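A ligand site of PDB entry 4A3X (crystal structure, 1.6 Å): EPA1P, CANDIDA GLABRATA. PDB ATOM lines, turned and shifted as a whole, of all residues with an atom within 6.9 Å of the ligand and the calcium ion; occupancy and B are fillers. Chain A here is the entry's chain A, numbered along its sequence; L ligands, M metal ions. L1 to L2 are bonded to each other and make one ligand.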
ATOM      1  N   TRP A  40      30.785  17.254  21.895  1.00  0.00           N
ATOM      2  CA  TRP A  40      30.780  16.742  23.267  1.00  0.00           C
ATOM      3  C   TRP A  40      31.223  15.289  23.347  1.00  0.00           C
ATOM      4  O   TRP A  40      31.019  14.475  22.381  1.00  0.00           O
ATOM      5  CB  TRP A  40      29.391  16.944  23.893  1.00  0.00           C
ATOM      6  CG  TRP A  40      28.200  16.528  23.137  1.00  0.00           C
ATOM      7  CD1 TRP A  40      27.383  17.315  22.353  1.00  0.00           C
ATOM      8  CD2 TRP A  40      27.618  15.195  23.080  1.00  0.00           C
ATOM      9  NE1 TRP A  40      26.325  16.599  21.883  1.00  0.00           N
ATOM     10  CE2 TRP A  40      26.460  15.273  22.285  1.00  0.00           C
ATOM     11  CE3 TRP A  40      27.951  13.980  23.724  1.00  0.00           C
ATOM     12  CZ2 TRP A  40      25.603  14.172  22.043  1.00  0.00           C
ATOM     13  CZ3 TRP A  40      27.165  12.859  23.485  1.00  0.00           C
ATOM     14  CH2 TRP A  40      25.968  12.977  22.668  1.00  0.00           C
ATOM     15  N   TYR A  44      30.576  10.344  29.380  1.00  0.00           N
ATOM     16  CA  TYR A  44      29.734  10.448  30.541  1.00  0.00           C
ATOM     17  C   TYR A  44      28.682   9.384  30.634  1.00  0.00           C
ATOM     18  O   TYR A  44      28.196   9.100  31.701  1.00  0.00           O
ATOM     19  CB  TYR A  44      29.083  11.839  30.680  1.00  0.00           C
ATOM     20  CG  TYR A  44      27.861  12.115  29.787  1.00  0.00           C
ATOM     21  CD1 TYR A  44      28.026  12.255  28.422  1.00  0.00           C
ATOM     22  CD2 TYR A  44      26.584  12.273  30.330  1.00  0.00           C
ATOM     23  CE1 TYR A  44      26.971  12.509  27.566  1.00  0.00           C
ATOM     24  CE2 TYR A  44      25.437  12.511  29.491  1.00  0.00           C
ATOM     25  CZ  TYR A  44      25.694  12.673  28.116  1.00  0.00           C
ATOM     26  OH  TYR A  44      24.576  12.877  27.291  1.00  0.00           O
ATOM     27  N   TYR A  73      20.737  26.563  37.757  1.00  0.00           N
ATOM     28  CA  TYR A  73      20.523  26.577  36.306  1.00  0.00           C
ATOM     29  C   TYR A  73      21.647  27.495  35.780  1.00  0.00           C
ATOM     30  O   TYR A  73      21.748  28.692  36.217  1.00  0.00           O
ATOM     31  CB  TYR A  73      19.097  27.116  35.842  1.00  0.00           C
ATOM     32  CG  TYR A  73      18.915  26.684  34.399  1.00  0.00           C
ATOM     33  CD1 TYR A  73      19.639  27.364  33.348  1.00  0.00           C
ATOM     34  CD2 TYR A  73      18.132  25.557  34.061  1.00  0.00           C
ATOM     35  CE1 TYR A  73      19.584  26.900  32.025  1.00  0.00           C
ATOM     36  CE2 TYR A  73      18.129  25.065  32.731  1.00  0.00           C
ATOM     37  CZ  TYR A  73      18.803  25.798  31.749  1.00  0.00           C
ATOM     38  OH  TYR A  73      18.713  25.307  30.466  1.00  0.00           O
ATOM     39  N   GLY A  79      27.402  26.739  22.013  1.00  0.00           N
ATOM     40  CA  GLY A  79      27.770  25.334  21.966  1.00  0.00           C
ATOM     41  C   GLY A  79      29.240  25.076  21.812  1.00  0.00           C
ATOM     42  O   GLY A  79      30.043  25.908  21.363  1.00  0.00           O
ATOM     43  N   CYS A  80      29.626  23.841  22.121  1.00  0.00           N
ATOM     44  CA  CYS A  80      30.937  23.343  21.774  1.00  0.00           C
ATOM     45  C   CYS A  80      32.081  24.193  22.334  1.00  0.00           C
ATOM     46  O   CYS A  80      33.200  24.189  21.804  1.00  0.00           O
ATOM     47  CB  CYS A  80      31.061  23.188  20.249  1.00  0.00           C
ATOM     48  SG  CYS A  80      29.851  22.025  19.563  1.00  0.00           S
ATOM     49  N   MET A  99      31.499  25.780  33.804  1.00  0.00           N
ATOM     50  CA  MET A  99      30.102  25.303  34.089  1.00  0.00           C
ATOM     51  C   MET A  99      29.414  24.638  32.936  1.00  0.00           C
ATOM     52  O   MET A  99      28.471  23.873  33.134  1.00  0.00           O
ATOM     53  CB  MET A  99      29.225  26.479  34.604  1.00  0.00           C
ATOM     54  CG  MET A  99      29.655  26.934  35.999  1.00  0.00           C
ATOM     55  SD  MET A  99      29.188  25.755  37.263  1.00  0.00           S
ATOM     56  CE  MET A  99      27.351  25.557  37.159  1.00  0.00           C
ATOM     57  N   THR A 100      29.950  24.886  31.721  1.00  0.00           N
ATOM     58  CA  THR A 100      29.437  24.163  30.480  1.00  0.00           C
ATOM     59  C   THR A 100      29.807  22.679  30.430  1.00  0.00           C
ATOM     60  O   THR A 100      29.212  21.898  29.668  1.00  0.00           O
ATOM     61  CB  THR A 100      30.046  24.801  29.245  1.00  0.00           C
ATOM     62  OG1 THR A 100      31.460  24.972  29.509  1.00  0.00           O
ATOM     63  CG2 THR A 100      29.412  26.229  28.934  1.00  0.00           C
ATOM     64  N   ASP A 125      20.565  18.592  33.740  1.00  0.00           N
ATOM     65  CA  ASP A 125      21.141  18.713  32.402  1.00  0.00           C
ATOM     66  C   ASP A 125      22.651  18.734  32.731  1.00  0.00           C
ATOM     67  O   ASP A 125      23.123  19.678  33.317  1.00  0.00           O
ATOM     68  CB  ASP A 125      20.669  20.062  31.796  1.00  0.00           C
ATOM     69  CG  ASP A 125      21.407  20.415  30.481  1.00  0.00           C
ATOM     70  OD1 ASP A 125      22.368  19.684  30.158  1.00  0.00           O
ATOM     71  OD2 ASP A 125      20.896  21.376  29.792  1.00  0.00           O
ATOM     72  N   ASP A 126      23.403  17.682  32.449  1.00  0.00           N
ATOM     73  CA  ASP A 126      23.010  16.497  31.616  1.00  0.00           C
ATOM     74  C   ASP A 126      22.612  15.267  32.370  1.00  0.00           C
ATOM     75  O   ASP A 126      21.800  14.520  31.870  1.00  0.00           O
ATOM     76  CB  ASP A 126      24.156  16.093  30.663  1.00  0.00           C
ATOM     77  CG  ASP A 126      24.221  17.023  29.510  1.00  0.00           C
ATOM     78  OD1 ASP A 126      23.445  16.873  28.458  1.00  0.00           O
ATOM     79  OD2 ASP A 126      24.901  18.074  29.567  1.00  0.00           O
ATOM     80  N   TRP A 159      19.352  14.260  30.595  1.00  0.00           N
ATOM     81  CA  TRP A 159      18.727  15.213  29.699  1.00  0.00           C
ATOM     82  C   TRP A 159      18.609  14.607  28.268  1.00  0.00           C
ATOM     83  O   TRP A 159      19.521  13.921  27.765  1.00  0.00           O
ATOM     84  CB  TRP A 159      19.621  16.466  29.623  1.00  0.00           C
ATOM     85  CG  TRP A 159      18.962  17.519  28.731  1.00  0.00           C
ATOM     86  CD1 TRP A 159      18.079  18.509  29.106  1.00  0.00           C
ATOM     87  CD2 TRP A 159      19.153  17.636  27.335  1.00  0.00           C
ATOM     88  NE1 TRP A 159      17.686  19.274  27.944  1.00  0.00           N
ATOM     89  CE2 TRP A 159      18.259  18.645  26.864  1.00  0.00           C
ATOM     90  CE3 TRP A 159      19.862  16.876  26.395  1.00  0.00           C
ATOM     91  CZ2 TRP A 159      18.181  19.012  25.460  1.00  0.00           C
ATOM     92  CZ3 TRP A 159      19.768  17.224  25.040  1.00  0.00           C
ATOM     93  CH2 TRP A 159      18.918  18.273  24.608  1.00  0.00           C
ATOM     94  N   TYR A 184      26.912  13.978  39.148  1.00  0.00           N
ATOM     95  CA  TYR A 184      26.333  14.902  38.217  1.00  0.00           C
ATOM     96  C   TYR A 184      27.360  15.117  37.119  1.00  0.00           C
ATOM     97  O   TYR A 184      28.606  15.164  37.375  1.00  0.00           O
ATOM     98  CB  TYR A 184      26.147  16.297  38.961  1.00  0.00           C
ATOM     99  CG  TYR A 184      25.892  17.437  37.975  1.00  0.00           C
ATOM    100  CD1 TYR A 184      24.582  17.553  37.401  1.00  0.00           C
ATOM    101  CD2 TYR A 184      26.936  18.248  37.466  1.00  0.00           C
ATOM    102  CE1 TYR A 184      24.295  18.556  36.382  1.00  0.00           C
ATOM    103  CE2 TYR A 184      26.666  19.182  36.483  1.00  0.00           C
ATOM    104  CZ  TYR A 184      25.357  19.373  35.961  1.00  0.00           C
ATOM    105  OH  TYR A 184      25.254  20.265  34.945  1.00  0.00           O
ATOM    106  N   ASN A 185      26.862  15.280  35.879  1.00  0.00           N
ATOM    107  CA  ASN A 185      27.740  15.769  34.781  1.00  0.00           C
ATOM    108  C   ASN A 185      27.036  16.783  33.864  1.00  0.00           C
ATOM    109  O   ASN A 185      25.803  16.672  33.592  1.00  0.00           O
ATOM    110  CB  ASN A 185      28.164  14.546  33.880  1.00  0.00           C
ATOM    111  CG  ASN A 185      28.857  14.977  32.589  1.00  0.00           C
ATOM    112  OD1 ASN A 185      28.240  15.048  31.510  1.00  0.00           O
ATOM    113  ND2 ASN A 185      30.153  15.307  32.714  1.00  0.00           N
ATOM    114  N   ASN A 186      27.817  17.762  33.396  1.00  0.00           N
ATOM    115  CA  ASN A 186      27.416  18.621  32.278  1.00  0.00           C
ATOM    116  C   ASN A 186      28.335  18.313  31.103  1.00  0.00           C
ATOM    117  O   ASN A 186      29.558  18.412  31.296  1.00  0.00           O
ATOM    118  CB  ASN A 186      27.422  20.129  32.605  1.00  0.00           C
ATOM    119  CG  ASN A 186      26.734  20.957  31.522  1.00  0.00           C
ATOM    120  OD1 ASN A 186      26.207  20.340  30.523  1.00  0.00           O
ATOM    121  ND2 ASN A 186      26.765  22.324  31.618  1.00  0.00           N
ATOM    122  N   ARG A 187      27.772  17.926  29.943  1.00  0.00           N
ATOM    123  CA  ARG A 187      28.614  17.600  28.745  1.00  0.00           C
ATOM    124  C   ARG A 187      28.923  18.791  27.838  1.00  0.00           C
ATOM    125  O   ARG A 187      29.910  18.744  27.093  1.00  0.00           O
ATOM    126  CB  ARG A 187      27.955  16.454  27.932  1.00  0.00           C
ATOM    127  CG  ARG A 187      26.881  17.024  26.927  1.00  0.00           C
ATOM    128  CD  ARG A 187      25.943  15.882  26.397  1.00  0.00           C
ATOM    129  NE  ARG A 187      25.005  16.513  25.421  1.00  0.00           N
ATOM    130  CZ  ARG A 187      24.099  15.793  24.706  1.00  0.00           C
ATOM    131  NH1 ARG A 187      23.949  14.481  24.970  1.00  0.00           N
ATOM    132  NH2 ARG A 187      23.306  16.401  23.779  1.00  0.00           N
ATOM    133  N   GLU A 188      28.134  19.880  27.934  1.00  0.00           N
ATOM    134  CA  GLU A 188      28.198  20.992  26.985  1.00  0.00           C
ATOM    135  C   GLU A 188      27.076  21.956  27.336  1.00  0.00           C
ATOM    136  O   GLU A 188      26.022  21.487  27.774  1.00  0.00           O
ATOM    137  CB  GLU A 188      27.891  20.430  25.519  1.00  0.00           C
ATOM    138  CG  GLU A 188      28.080  21.549  24.536  1.00  0.00           C
ATOM    139  CD  GLU A 188      27.376  21.291  23.192  1.00  0.00           C
ATOM    140  OE1 GLU A 188      26.409  20.428  23.057  1.00  0.00           O
ATOM    141  OE2 GLU A 188      27.805  21.957  22.246  1.00  0.00           O
ATOM    142  N   TYR A 189      27.256  23.257  26.999  1.00  0.00           N
ATOM    143  CA  TYR A 189      26.135  24.217  26.958  1.00  0.00           C
ATOM    144  C   TYR A 189      25.513  24.368  28.360  1.00  0.00           C
ATOM    145  O   TYR A 189      26.197  24.345  29.381  1.00  0.00           O
ATOM    146  CB  TYR A 189      25.089  23.840  25.862  1.00  0.00           C
ATOM    147  CG  TYR A 189      24.273  25.041  25.369  1.00  0.00           C
ATOM    148  CD1 TYR A 189      24.932  26.085  24.745  1.00  0.00           C
ATOM    149  CD2 TYR A 189      22.896  25.009  25.409  1.00  0.00           C
ATOM    150  CE1 TYR A 189      24.239  27.162  24.262  1.00  0.00           C
ATOM    151  CE2 TYR A 189      22.156  26.133  24.895  1.00  0.00           C
ATOM    152  CZ  TYR A 189      22.870  27.207  24.384  1.00  0.00           C
ATOM    153  OH  TYR A 189      22.263  28.306  23.782  1.00  0.00           O
ATOM    154  N   ASP A 190      24.168  24.517  28.429  1.00  0.00           N
ATOM    155  CA  ASP A 190      23.541  24.765  29.689  1.00  0.00           C
ATOM    156  C   ASP A 190      23.769  23.582  30.660  1.00  0.00           C
ATOM    157  O   ASP A 190      23.931  22.358  30.296  1.00  0.00           O
ATOM    158  CB  ASP A 190      22.000  24.961  29.551  1.00  0.00           C
ATOM    159  CG  ASP A 190      21.635  26.243  28.842  1.00  0.00           C
ATOM    160  OD1 ASP A 190      22.522  26.990  28.381  1.00  0.00           O
ATOM    161  OD2 ASP A 190      20.383  26.466  28.720  1.00  0.00           O
ATOM    162  N   GLY A 191      23.720  23.950  31.954  1.00  0.00           N
ATOM    163  CA  GLY A 191      23.676  22.871  32.976  1.00  0.00           C
ATOM    164  C   GLY A 191      22.608  23.131  33.983  1.00  0.00           C
ATOM    165  O   GLY A 191      22.332  24.314  34.299  1.00  0.00           O
ATOM    166  N   ALA A 192      22.111  22.083  34.607  1.00  0.00           N
ATOM    167  CA  ALA A 192      21.075  22.266  35.616  1.00  0.00           C
ATOM    168  C   ALA A 192      21.027  21.074  36.537  1.00  0.00           C
ATOM    169  O   ALA A 192      21.263  19.920  36.135  1.00  0.00           O
ATOM    170  CB  ALA A 192      19.705  22.405  34.961  1.00  0.00           C
HETATM  171  C1  LIG L   1      22.621  21.922  21.930  1.00  0.00           C
HETATM  172  O1  LIG L   1      23.375  21.809  23.202  1.00  0.00           O
HETATM  173  C1  LG2 L   2      22.664  21.032  24.167  1.00  0.00           C
HETATM  174  C2  LG2 L   2      23.625  20.256  25.083  1.00  0.00           C
HETATM  175  C3  LG2 L   2      22.863  19.551  26.188  1.00  0.00           C
HETATM  176  C4  LG2 L   2      21.843  20.436  26.858  1.00  0.00           C
HETATM  177  C5  LG2 L   2      20.967  21.098  25.781  1.00  0.00           C
HETATM  178  C6  LG2 L   2      19.926  22.025  26.446  1.00  0.00           C
HETATM  179  O1  LG2 L   2      24.311  19.209  24.299  1.00  0.00           O
HETATM  180  O2  LG2 L   2      23.840  19.110  27.136  1.00  0.00           O
HETATM  181  O3  LG2 L   2      22.511  21.452  27.623  1.00  0.00           O
HETATM  182  O4  LG2 L   2      21.775  21.890  24.920  1.00  0.00           O
HETATM  183  O5  LG2 L   2      19.350  22.894  25.425  1.00  0.00           O
HETATM  184 CA    CA M   1      24.349  20.413  29.057  1.00  0.00          CA
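OE1 of Glu 188 lies within hydrogen-bond range of O1 of LG2 L2 (2.7 Å). NE of Arg 187 lies within hydrogen-bond range of O1 of LG2 L2, 3.0 Å away.
N of Asp 125 is in hydrogen-bond range of O of Ala 192 (2.8 Å). The backbone NH (N) of Glu 188 lies within hydrogen-bond range of the backbone carbonyl oxygen (O) of Thr 100 (2.9 Å). ND2 of Asn 186 sits at hydrogen-bond distance from O of Thr 100, 3.2 Å away. The side-chain hydroxyl of Tyr 44 sits at hydrogen-bond distance from the guanidinium group of Arg 187, at 2.9 Å. The side-chain hydroxyl (OH) of Tyr 73 sits at hydrogen-bond distance from the side-chain carboxylate (OD2) of Asp 190. The backbone carbonyl oxygen (O) of Asp 126 is in hydrogen-bond range of the backbone NH (N) of Trp 159. O of Met 99 lies within hydrogen-bond range of ND2 of Asn 186, 2.8 Å away. The backbone carbonyl oxygen (O) of Asn 185 sits at hydrogen-bond distance from the backbone NH (N) of Asp 126 (2.8 Å).
Residues that only touch the ligand: Trp 159 (3.5 Å) and Tyr 189 (3.4 Å).
Of the 19 residues printed, 5 come within 4 Å of the calcium ion.
The calcium ion is bound by O of Asp 190 (2.3 Å), O of Glu 188 (2.4 Å), OD1 of Asn 186 (2.4 Å), O2 of LG2 L2 (2.4 Å), OD1 of Asp 125 (2.4 Å), OD2 of Asp 126 (2.5 Å) and O3 of LG2 L2 (2.6 Å). The calcium ion has seven donor atoms within binding distance.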
